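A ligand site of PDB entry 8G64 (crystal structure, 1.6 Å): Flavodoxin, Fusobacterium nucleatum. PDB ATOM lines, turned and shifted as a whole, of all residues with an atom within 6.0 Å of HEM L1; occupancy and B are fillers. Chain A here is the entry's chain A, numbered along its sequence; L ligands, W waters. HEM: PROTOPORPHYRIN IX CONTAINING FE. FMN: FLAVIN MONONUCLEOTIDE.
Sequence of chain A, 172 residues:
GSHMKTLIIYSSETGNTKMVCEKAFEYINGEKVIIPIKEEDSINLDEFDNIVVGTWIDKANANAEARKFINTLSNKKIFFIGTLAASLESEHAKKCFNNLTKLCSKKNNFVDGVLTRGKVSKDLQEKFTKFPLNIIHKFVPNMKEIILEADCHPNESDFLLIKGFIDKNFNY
FE of HEM L1 is bound by NE2 of His 137, 2.2 Å away.
ND1 of His 92 sits at hydrogen-bond distance from O2D of HEM L1 (2.8 Å).
An oxygen (O2D) of HEM L1 lies within salt-bridge range of the side-chain amino group (NZ) of Lys 95 (3.0 Å).
N3 of FMN L2 sits at hydrogen-bond distance from NE2 of His 92.
N of Ala 85 is in hydrogen-bond range of O2 of FMN L2 (3.2 Å).
N of Lys 59 is in hydrogen-bond range of N5 of FMN L2.
N of Ala 86 lies within hydrogen-bond range of O2 of FMN L2 (2.9 Å).
O4 of FMN L2 lies within hydrogen-bond range of N of Ala 60 (3.1 Å).
A ring nitrogen (ND1) of His 137 lies within hydrogen-bond range of the backbone carbonyl oxygen (O) of Leu 133 (2.9 Å).
The side-chain carboxylate (OD1) of Asp 58 lies within salt-bridge range of the side-chain amino group (NZ) of Lys 59 (2.9 Å).
CG of Lys 59 touches CHB of HEM L1, 3.7 Å away.
CB of Ala 85 touches CBC of HEM L1, at 3.3 Å.
Ala 86 touches HEM L1 (N to CBC, 3.9 Å).
Leu 124 touches HEM L1.
Phe 128 touches HEM L1.
Leu 133 touches HEM L1.
CG2 of Ile 136 touches C3A of HEM L1 (3.4 Å).
CG1 of Val 140 touches CMD of HEM L1, at 3.5 Å.
Met 143 touches HEM L1 (CE to CAC, 3.7 Å).
Ile 146 touches HEM L1 (CG2 to CBC, 3.7 Å).
13 residues have an atom within 4 Å of HEM L1: Lys 59, Ala 85, Ala 86, His 92, Lys 95, Leu 124, Phe 128, Leu 133, Ile 136, His 137, Val 140, Met 143 and Ile 146.
Water W6 bridges O1A of HEM L1 (2.6 Å) and NZ of Lys 95 (3.5 Å).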
ATOM      1  N   ASP A  58      -9.806  23.920  13.690  1.00  0.00           N
ATOM      2  CA  ASP A  58      -8.395  24.031  14.018  1.00  0.00           C
ATOM      3  C   ASP A  58      -7.628  23.526  12.795  1.00  0.00           C
ATOM      4  O   ASP A  58      -7.664  22.334  12.477  1.00  0.00           O
ATOM      5  CB  ASP A  58      -8.072  23.205  15.278  1.00  0.00           C
ATOM      6  CG  ASP A  58      -6.614  23.306  15.710  1.00  0.00           C
ATOM      7  OD1 ASP A  58      -5.780  23.781  14.913  1.00  0.00           O
ATOM      8  OD2 ASP A  58      -6.313  22.889  16.840  1.00  0.00           O
ATOM      9  N   LYS A  59      -6.963  24.428  12.081  1.00  0.00           N
ATOM     10  CA  LYS A  59      -6.214  24.072  10.875  1.00  0.00           C
ATOM     11  C   LYS A  59      -7.076  23.282   9.893  1.00  0.00           C
ATOM     12  O   LYS A  59      -6.723  22.200   9.415  1.00  0.00           O
ATOM     13  CB  LYS A  59      -4.933  23.274  11.197  1.00  0.00           C
ATOM     14  CG  LYS A  59      -3.907  23.973  12.042  1.00  0.00           C
ATOM     15  CD  LYS A  59      -2.812  22.969  12.488  1.00  0.00           C
ATOM     16  CE  LYS A  59      -3.115  22.322  13.845  1.00  0.00           C
ATOM     17  NZ  LYS A  59      -2.919  23.244  14.998  1.00  0.00           N
ATOM     18  N   ALA A  60      -8.245  23.841   9.595  1.00  0.00           N
ATOM     19  CA  ALA A  60      -9.213  23.329   8.622  1.00  0.00           C
ATOM     20  C   ALA A  60      -9.899  22.039   9.040  1.00  0.00           C
ATOM     21  O   ALA A  60     -10.598  21.424   8.217  1.00  0.00           O
ATOM     22  CB  ALA A  60      -8.574  23.116   7.248  1.00  0.00           C
ATOM     23  N   ALA A  85     -13.301  31.123  11.897  1.00  0.00           N
ATOM     24  CA  ALA A  85     -13.166  32.566  11.713  1.00  0.00           C
ATOM     25  C   ALA A  85     -13.210  33.003  10.260  1.00  0.00           C
ATOM     26  O   ALA A  85     -13.486  34.176   9.981  1.00  0.00           O
ATOM     27  CB  ALA A  85     -11.867  33.054  12.362  1.00  0.00           C
ATOM     28  N   ALA A  86     -12.913  32.104   9.322  1.00  0.00           N
ATOM     29  CA  ALA A  86     -12.920  32.464   7.920  1.00  0.00           C
ATOM     30  C   ALA A  86     -14.322  32.869   7.458  1.00  0.00           C
ATOM     31  O   ALA A  86     -15.336  32.537   8.082  1.00  0.00           O
ATOM     32  CB  ALA A  86     -12.442  31.301   7.065  1.00  0.00           C
ATOM     33  N   GLU A  91     -13.457  29.468   0.005  1.00  0.00           N
ATOM     34  CA  GLU A  91     -13.041  28.100  -0.326  1.00  0.00           C
ATOM     35  C   GLU A  91     -12.517  27.385   0.917  1.00  0.00           C
ATOM     36  O   GLU A  91     -12.707  26.180   1.056  1.00  0.00           O
ATOM     37  CB  GLU A  91     -11.971  28.116  -1.413  1.00  0.00           C
ATOM     38  CG  GLU A  91     -12.523  28.441  -2.793  1.00  0.00           C
ATOM     39  CD  GLU A  91     -13.557  27.409  -3.257  1.00  0.00           C
ATOM     40  OE1 GLU A  91     -13.273  26.194  -3.134  1.00  0.00           O
ATOM     41  OE2 GLU A  91     -14.626  27.813  -3.755  1.00  0.00           O
ATOM     42  N   HIS A  92     -11.872  28.125   1.820  1.00  0.00           N
ATOM     43  CA  HIS A  92     -11.434  27.534   3.077  1.00  0.00           C
ATOM     44  C   HIS A  92     -12.615  26.953   3.846  1.00  0.00           C
ATOM     45  O   HIS A  92     -12.558  25.821   4.339  1.00  0.00           O
ATOM     46  CB  HIS A  92     -10.698  28.568   3.932  1.00  0.00           C
ATOM     47  CG  HIS A  92     -10.185  28.049   5.234  1.00  0.00           C
ATOM     48  ND1 HIS A  92      -9.026  27.307   5.337  1.00  0.00           N
ATOM     49  CD2 HIS A  92     -10.666  28.172   6.491  1.00  0.00           C
ATOM     50  CE1 HIS A  92      -8.817  27.004   6.598  1.00  0.00           C
ATOM     51  NE2 HIS A  92      -9.808  27.486   7.322  1.00  0.00           N
ATOM     52  N   LYS A  95     -13.689  23.749   2.275  1.00  0.00           N
ATOM     53  CA  LYS A  95     -12.745  22.689   2.647  1.00  0.00           C
ATOM     54  C   LYS A  95     -13.022  22.189   4.059  1.00  0.00           C
ATOM     55  O   LYS A  95     -13.030  20.981   4.298  1.00  0.00           O
ATOM     56  CB  LYS A  95     -11.316  23.214   2.519  1.00  0.00           C
ATOM     57  CG  LYS A  95     -10.234  22.391   3.185  1.00  0.00           C
ATOM     58  CD  LYS A  95      -8.882  23.103   3.061  1.00  0.00           C
ATOM     59  CE  LYS A  95      -7.742  22.305   3.672  1.00  0.00           C
ATOM     60  NZ  LYS A  95      -6.467  23.084   3.643  1.00  0.00           N
ATOM     61  N   VAL A 120     -11.871  35.372  16.309  1.00  0.00           N
ATOM     62  CA  VAL A 120     -10.569  34.863  16.718  1.00  0.00           C
ATOM     63  C   VAL A 120     -10.264  35.369  18.128  1.00  0.00           C
ATOM     64  O   VAL A 120     -10.462  36.556  18.433  1.00  0.00           O
ATOM     65  CB  VAL A 120      -9.482  35.302  15.719  1.00  0.00           C
ATOM     66  CG1 VAL A 120      -8.113  34.709  16.126  1.00  0.00           C
ATOM     67  CG2 VAL A 120      -9.855  34.905  14.288  1.00  0.00           C
ATOM     68  N   LEU A 124      -4.994  34.471  20.192  1.00  0.00           N
ATOM     69  CA  LEU A 124      -4.575  34.032  18.856  1.00  0.00           C
ATOM     70  C   LEU A 124      -4.337  35.232  17.945  1.00  0.00           C
ATOM     71  O   LEU A 124      -3.412  35.218  17.126  1.00  0.00           O
ATOM     72  CB  LEU A 124      -5.607  33.091  18.259  1.00  0.00           C
ATOM     73  CG  LEU A 124      -5.310  32.500  16.897  1.00  0.00           C
ATOM     74  CD1 LEU A 124      -3.942  31.881  16.835  1.00  0.00           C
ATOM     75  CD2 LEU A 124      -6.383  31.459  16.579  1.00  0.00           C
ATOM     76  N   PHE A 128      -0.809  35.771  15.991  1.00  0.00           N
ATOM     77  CA  PHE A 128      -0.779  35.923  14.540  1.00  0.00           C
ATOM     78  C   PHE A 128       0.249  36.966  14.093  1.00  0.00           C
ATOM     79  O   PHE A 128       0.635  36.936  12.977  1.00  0.00           O
ATOM     80  CB  PHE A 128      -2.165  36.269  13.937  1.00  0.00           C
ATOM     81  CG  PHE A 128      -2.753  35.165  13.130  1.00  0.00           C
ATOM     82  CD1 PHE A 128      -3.381  34.114  13.749  1.00  0.00           C
ATOM     83  CD2 PHE A 128      -2.687  35.183  11.753  1.00  0.00           C
ATOM     84  CE1 PHE A 128      -3.929  33.082  13.017  1.00  0.00           C
ATOM     85  CE2 PHE A 128      -3.223  34.170  11.014  1.00  0.00           C
ATOM     86  CZ  PHE A 128      -3.855  33.119  11.642  1.00  0.00           C
ATOM     87  N   LEU A 133       3.105  31.859  13.182  1.00  0.00           N
ATOM     88  CA  LEU A 133       1.830  32.045  12.492  1.00  0.00           C
ATOM     89  C   LEU A 133       1.894  33.180  11.465  1.00  0.00           C
ATOM     90  O   LEU A 133       1.258  33.090  10.410  1.00  0.00           O
ATOM     91  CB  LEU A 133       0.703  32.327  13.487  1.00  0.00           C
ATOM     92  CG  LEU A 133       0.292  31.172  14.385  1.00  0.00           C
ATOM     93  CD1 LEU A 133      -0.737  31.596  15.397  1.00  0.00           C
ATOM     94  CD2 LEU A 133      -0.235  29.997  13.573  1.00  0.00           C
ATOM     95  N   ILE A 136       3.493  31.755   8.415  1.00  0.00           N
ATOM     96  CA  ILE A 136       2.705  30.683   7.820  1.00  0.00           C
ATOM     97  C   ILE A 136       1.578  31.260   6.970  1.00  0.00           C
ATOM     98  O   ILE A 136       1.216  30.696   5.927  1.00  0.00           O
ATOM     99  CB  ILE A 136       2.176  29.746   8.918  1.00  0.00           C
ATOM    100  CG1 ILE A 136       3.328  28.884   9.452  1.00  0.00           C
ATOM    101  CG2 ILE A 136       1.030  28.901   8.401  1.00  0.00           C
ATOM    102  CD1 ILE A 136       2.993  28.137  10.739  1.00  0.00           C
ATOM    103  N   HIS A 137       1.009  32.377   7.408  1.00  0.00           N
ATOM    104  CA  HIS A 137      -0.140  32.988   6.740  1.00  0.00           C
ATOM    105  C   HIS A 137       0.229  34.189   5.888  1.00  0.00           C
ATOM    106  O   HIS A 137      -0.658  34.904   5.429  1.00  0.00           O
ATOM    107  CB  HIS A 137      -1.188  33.385   7.768  1.00  0.00           C
ATOM    108  CG  HIS A 137      -1.775  32.229   8.483  1.00  0.00           C
ATOM    109  ND1 HIS A 137      -1.183  31.672   9.603  1.00  0.00           N
ATOM    110  CD2 HIS A 137      -2.873  31.478   8.224  1.00  0.00           C
ATOM    111  CE1 HIS A 137      -1.903  30.650  10.014  1.00  0.00           C
ATOM    112  NE2 HIS A 137      -2.931  30.510   9.200  1.00  0.00           N
ATOM    113  N   VAL A 140      -1.634  34.192   2.647  1.00  0.00           N
ATOM    114  CA  VAL A 140      -3.073  33.956   2.680  1.00  0.00           C
ATOM    115  C   VAL A 140      -3.754  35.303   2.442  1.00  0.00           C
ATOM    116  O   VAL A 140      -3.585  36.242   3.241  1.00  0.00           O
ATOM    117  CB  VAL A 140      -3.509  33.336   4.018  1.00  0.00           C
ATOM    118  CG1 VAL A 140      -5.002  33.126   4.039  1.00  0.00           C
ATOM    119  CG2 VAL A 140      -2.792  32.010   4.224  1.00  0.00           C
ATOM    120  N   MET A 143      -5.947  38.314   5.028  1.00  0.00           N
ATOM    121  CA  MET A 143      -5.831  37.769   6.375  1.00  0.00           C
ATOM    122  C   MET A 143      -6.331  38.791   7.411  1.00  0.00           C
ATOM    123  O   MET A 143      -7.111  38.446   8.317  1.00  0.00           O
ATOM    124  CB  MET A 143      -4.352  37.410   6.703  1.00  0.00           C
ATOM    125  CG  MET A 143      -4.243  36.316   7.759  1.00  0.00           C
ATOM    126  SD  MET A 143      -5.000  34.749   7.462  1.00  0.00           S
ATOM    127  CE  MET A 143      -6.168  34.618   8.797  1.00  0.00           C
ATOM    128  N   ILE A 146     -10.174  39.259   7.189  1.00  0.00           N
ATOM    129  CA  ILE A 146     -10.885  38.065   7.635  1.00  0.00           C
ATOM    130  C   ILE A 146     -10.991  38.060   9.156  1.00  0.00           C
ATOM    131  O   ILE A 146     -12.050  37.786   9.728  1.00  0.00           O
ATOM    132  CB  ILE A 146     -10.195  36.794   7.122  1.00  0.00           C
ATOM    133  CG1 ILE A 146     -10.385  36.664   5.616  1.00  0.00           C
ATOM    134  CG2 ILE A 146     -10.743  35.573   7.866  1.00  0.00           C
ATOM    135  CD1 ILE A 146      -9.430  35.672   4.983  1.00  0.00           C
ATOM    136  N   ILE A 147      -9.876  38.354   9.823  1.00  0.00           N
ATOM    137  CA  ILE A 147      -9.879  38.333  11.277  1.00  0.00           C
ATOM    138  C   ILE A 147     -10.777  39.440  11.817  1.00  0.00           C
ATOM    139  O   ILE A 147     -11.582  39.216  12.727  1.00  0.00           O
ATOM    140  CB  ILE A 147      -8.443  38.454  11.817  1.00  0.00           C
ATOM    141  CG1 ILE A 147      -7.649  37.195  11.471  1.00  0.00           C
ATOM    142  CG2 ILE A 147      -8.455  38.705  13.326  1.00  0.00           C
ATOM    143  CD1 ILE A 147      -6.147  37.388  11.582  1.00  0.00           C
HETATM  144  CHA HEM L   1      -3.163  28.004   6.053  1.00  0.00           C
HETATM  145  CHB HEM L   1      -1.971  26.742  10.592  1.00  0.00           C
HETATM  146  CHC HEM L   1      -5.311  29.816  12.286  1.00  0.00           C
HETATM  147  CHD HEM L   1      -6.949  30.521   7.805  1.00  0.00           C
HETATM  148  C1A HEM L   1      -2.532  27.423   7.135  1.00  0.00           C
HETATM  149  C2A HEM L   1      -1.398  26.522   7.077  1.00  0.00           C
HETATM  150  C3A HEM L   1      -1.062  26.176   8.324  1.00  0.00           C
HETATM  151  C4A HEM L   1      -1.983  26.827   9.225  1.00  0.00           C
HETATM  152  CMA HEM L   1       0.066  25.233   8.790  1.00  0.00           C
HETATM  153  CAA HEM L   1      -0.706  26.059   5.770  1.00  0.00           C
HETATM  154  CBA HEM L   1      -1.407  24.822   5.228  1.00  0.00           C
HETATM  155  CGA HEM L   1      -0.959  23.599   5.991  1.00  0.00           C
HETATM  156  O1A HEM L   1      -1.827  22.899   6.574  1.00  0.00           O
HETATM  157  O2A HEM L   1       0.272  23.325   6.039  1.00  0.00           O
HETATM  158  C1B HEM L   1      -2.765  27.474  11.450  1.00  0.00           C
HETATM  159  C2B HEM L   1      -2.689  27.485  12.889  1.00  0.00           C
HETATM  160  C3B HEM L   1      -3.616  28.328  13.359  1.00  0.00           C
HETATM  161  C4B HEM L   1      -4.287  28.899  12.220  1.00  0.00           C
HETATM  162  CMB HEM L   1      -1.699  26.601  13.685  1.00  0.00           C
HETATM  163  CAB HEM L   1      -3.937  28.722  14.809  1.00  0.00           C
HETATM  164  CBB HEM L   1      -3.093  28.406  15.827  1.00  0.00           C
HETATM  165  C1C HEM L   1      -6.054  30.247  11.213  1.00  0.00           C
HETATM  166  C2C HEM L   1      -7.206  31.141  11.308  1.00  0.00           C
HETATM  167  C3C HEM L   1      -7.658  31.320  10.059  1.00  0.00           C
HETATM  168  C4C HEM L   1      -6.821  30.573   9.165  1.00  0.00           C
HETATM  169  CMC HEM L   1      -7.726  31.735  12.640  1.00  0.00           C
HETATM  170  CAC HEM L   1      -8.843  32.180   9.577  1.00  0.00           C
HETATM  171  CBC HEM L   1      -9.282  33.219  10.303  1.00  0.00           C
HETATM  172  C1D HEM L   1      -6.050  29.896   6.959  1.00  0.00           C
HETATM  173  C2D HEM L   1      -6.159  29.888   5.518  1.00  0.00           C
HETATM  174  C3D HEM L   1      -5.142  29.184   5.020  1.00  0.00           C
HETATM  175  C4D HEM L   1      -4.323  28.758   6.142  1.00  0.00           C
HETATM  176  CMD HEM L   1      -7.296  30.541   4.724  1.00  0.00           C
HETATM  177  CAD HEM L   1      -4.858  28.899   3.529  1.00  0.00           C
HETATM  178  CBD HEM L   1      -5.020  27.395   3.267  1.00  0.00           C
HETATM  179  CGD HEM L   1      -6.466  26.987   3.404  1.00  0.00           C
HETATM  180  O1D HEM L   1      -7.344  27.576   2.742  1.00  0.00           O
HETATM  181  O2D HEM L   1      -6.764  26.049   4.160  1.00  0.00           O
HETATM  182  NA  HEM L   1      -2.838  27.604   8.465  1.00  0.00           N
HETATM  183  NB  HEM L   1      -3.757  28.349  11.060  1.00  0.00           N
HETATM  184  NC  HEM L   1      -5.865  29.931   9.891  1.00  0.00           N
HETATM  185  ND  HEM L   1      -4.906  29.185   7.343  1.00  0.00           N
HETATM  186 FE   HEM L   1      -4.309  28.786   9.139  1.00  0.00          FE
HETATM  187  N1  FMN L   2     -10.486  29.451  11.903  1.00  0.00           N
HETATM  188  C2  FMN L   2     -10.536  29.187  10.564  1.00  0.00           C
HETATM  189  O2  FMN L   2     -11.348  29.733   9.833  1.00  0.00           O
HETATM  190  N3  FMN L   2      -9.668  28.255  10.045  1.00  0.00           N
HETATM  191  C4  FMN L   2      -8.718  27.655  10.809  1.00  0.00           C
HETATM  192  O4  FMN L   2      -7.975  26.814  10.270  1.00  0.00           O
HETATM  193  C4A FMN L   2      -8.671  27.942  12.156  1.00  0.00           C
HETATM  194  N5  FMN L   2      -7.731  27.331  12.961  1.00  0.00           N
HETATM  195  C5A FMN L   2      -7.693  27.622  14.305  1.00  0.00           C
HETATM  196  C6  FMN L   2      -6.748  26.998  15.111  1.00  0.00           C
HETATM  197  C7  FMN L   2      -6.709  27.277  16.467  1.00  0.00           C
HETATM  198  C7M FMN L   2      -5.686  26.591  17.328  1.00  0.00           C
HETATM  199  C8  FMN L   2      -7.586  28.198  17.026  1.00  0.00           C
HETATM  200  C8M FMN L   2      -7.556  28.489  18.506  1.00  0.00           C
HETATM  201  C9  FMN L   2      -8.536  28.813  16.219  1.00  0.00           C
HETATM  202  C9A FMN L   2      -8.583  28.538  14.859  1.00  0.00           C
HETATM  203  N10 FMN L   2      -9.532  29.153  14.052  1.00  0.00           N
HETATM  204  C10 FMN L   2      -9.565  28.849  12.710  1.00  0.00           C
HETATM  205  C1' FMN L   2     -10.536  30.095  14.626  1.00  0.00           C
HETATM  206  C2' FMN L   2     -11.609  29.272  15.364  1.00  0.00           C
HETATM  207  O2' FMN L   2     -12.095  28.197  14.572  1.00  0.00           O
HETATM  208  C3' FMN L   2     -12.815  30.145  15.771  1.00  0.00           C
HETATM  209  O3' FMN L   2     -12.296  31.309  16.410  1.00  0.00           O
HETATM  210  C4' FMN L   2     -13.798  29.409  16.655  1.00  0.00           C
HETATM  211  O4' FMN L   2     -15.068  30.081  16.537  1.00  0.00           O
HETATM  212  C5' FMN L   2     -13.404  29.311  18.113  1.00  0.00           C
HETATM  213  O5' FMN L   2     -14.338  28.455  18.787  1.00  0.00           O
HETATM  214  P   FMN L   2     -14.572  28.468  20.356  1.00  0.00           P
HETATM  215  O1P FMN L   2     -13.312  27.901  20.977  1.00  0.00           O
HETATM  216  O2P FMN L   2     -14.804  29.921  20.772  1.00  0.00           O
HETATM  217  O3P FMN L   2     -15.807  27.610  20.544  1.00  0.00           O
HETATM  218  O   HOH W   1     -10.034  32.330   3.489  1.00  0.00           O
HETATM  219  O   HOH W   2      -8.189  29.309   0.699  1.00  0.00           O
HETATM  220  O   HOH W   3       2.093  22.005   7.385  1.00  0.00           O
HETATM  221  O   HOH W   4      -5.618  25.556   6.830  1.00  0.00           O
HETATM  222  O   HOH W   5       1.443  24.337   3.434  1.00  0.00           O
HETATM  223  O   HOH W   6      -4.384  23.352   6.426  1.00  0.00           O
HETATM  224  O   HOH W   7      -5.584  27.027   9.076  1.00  0.00           O
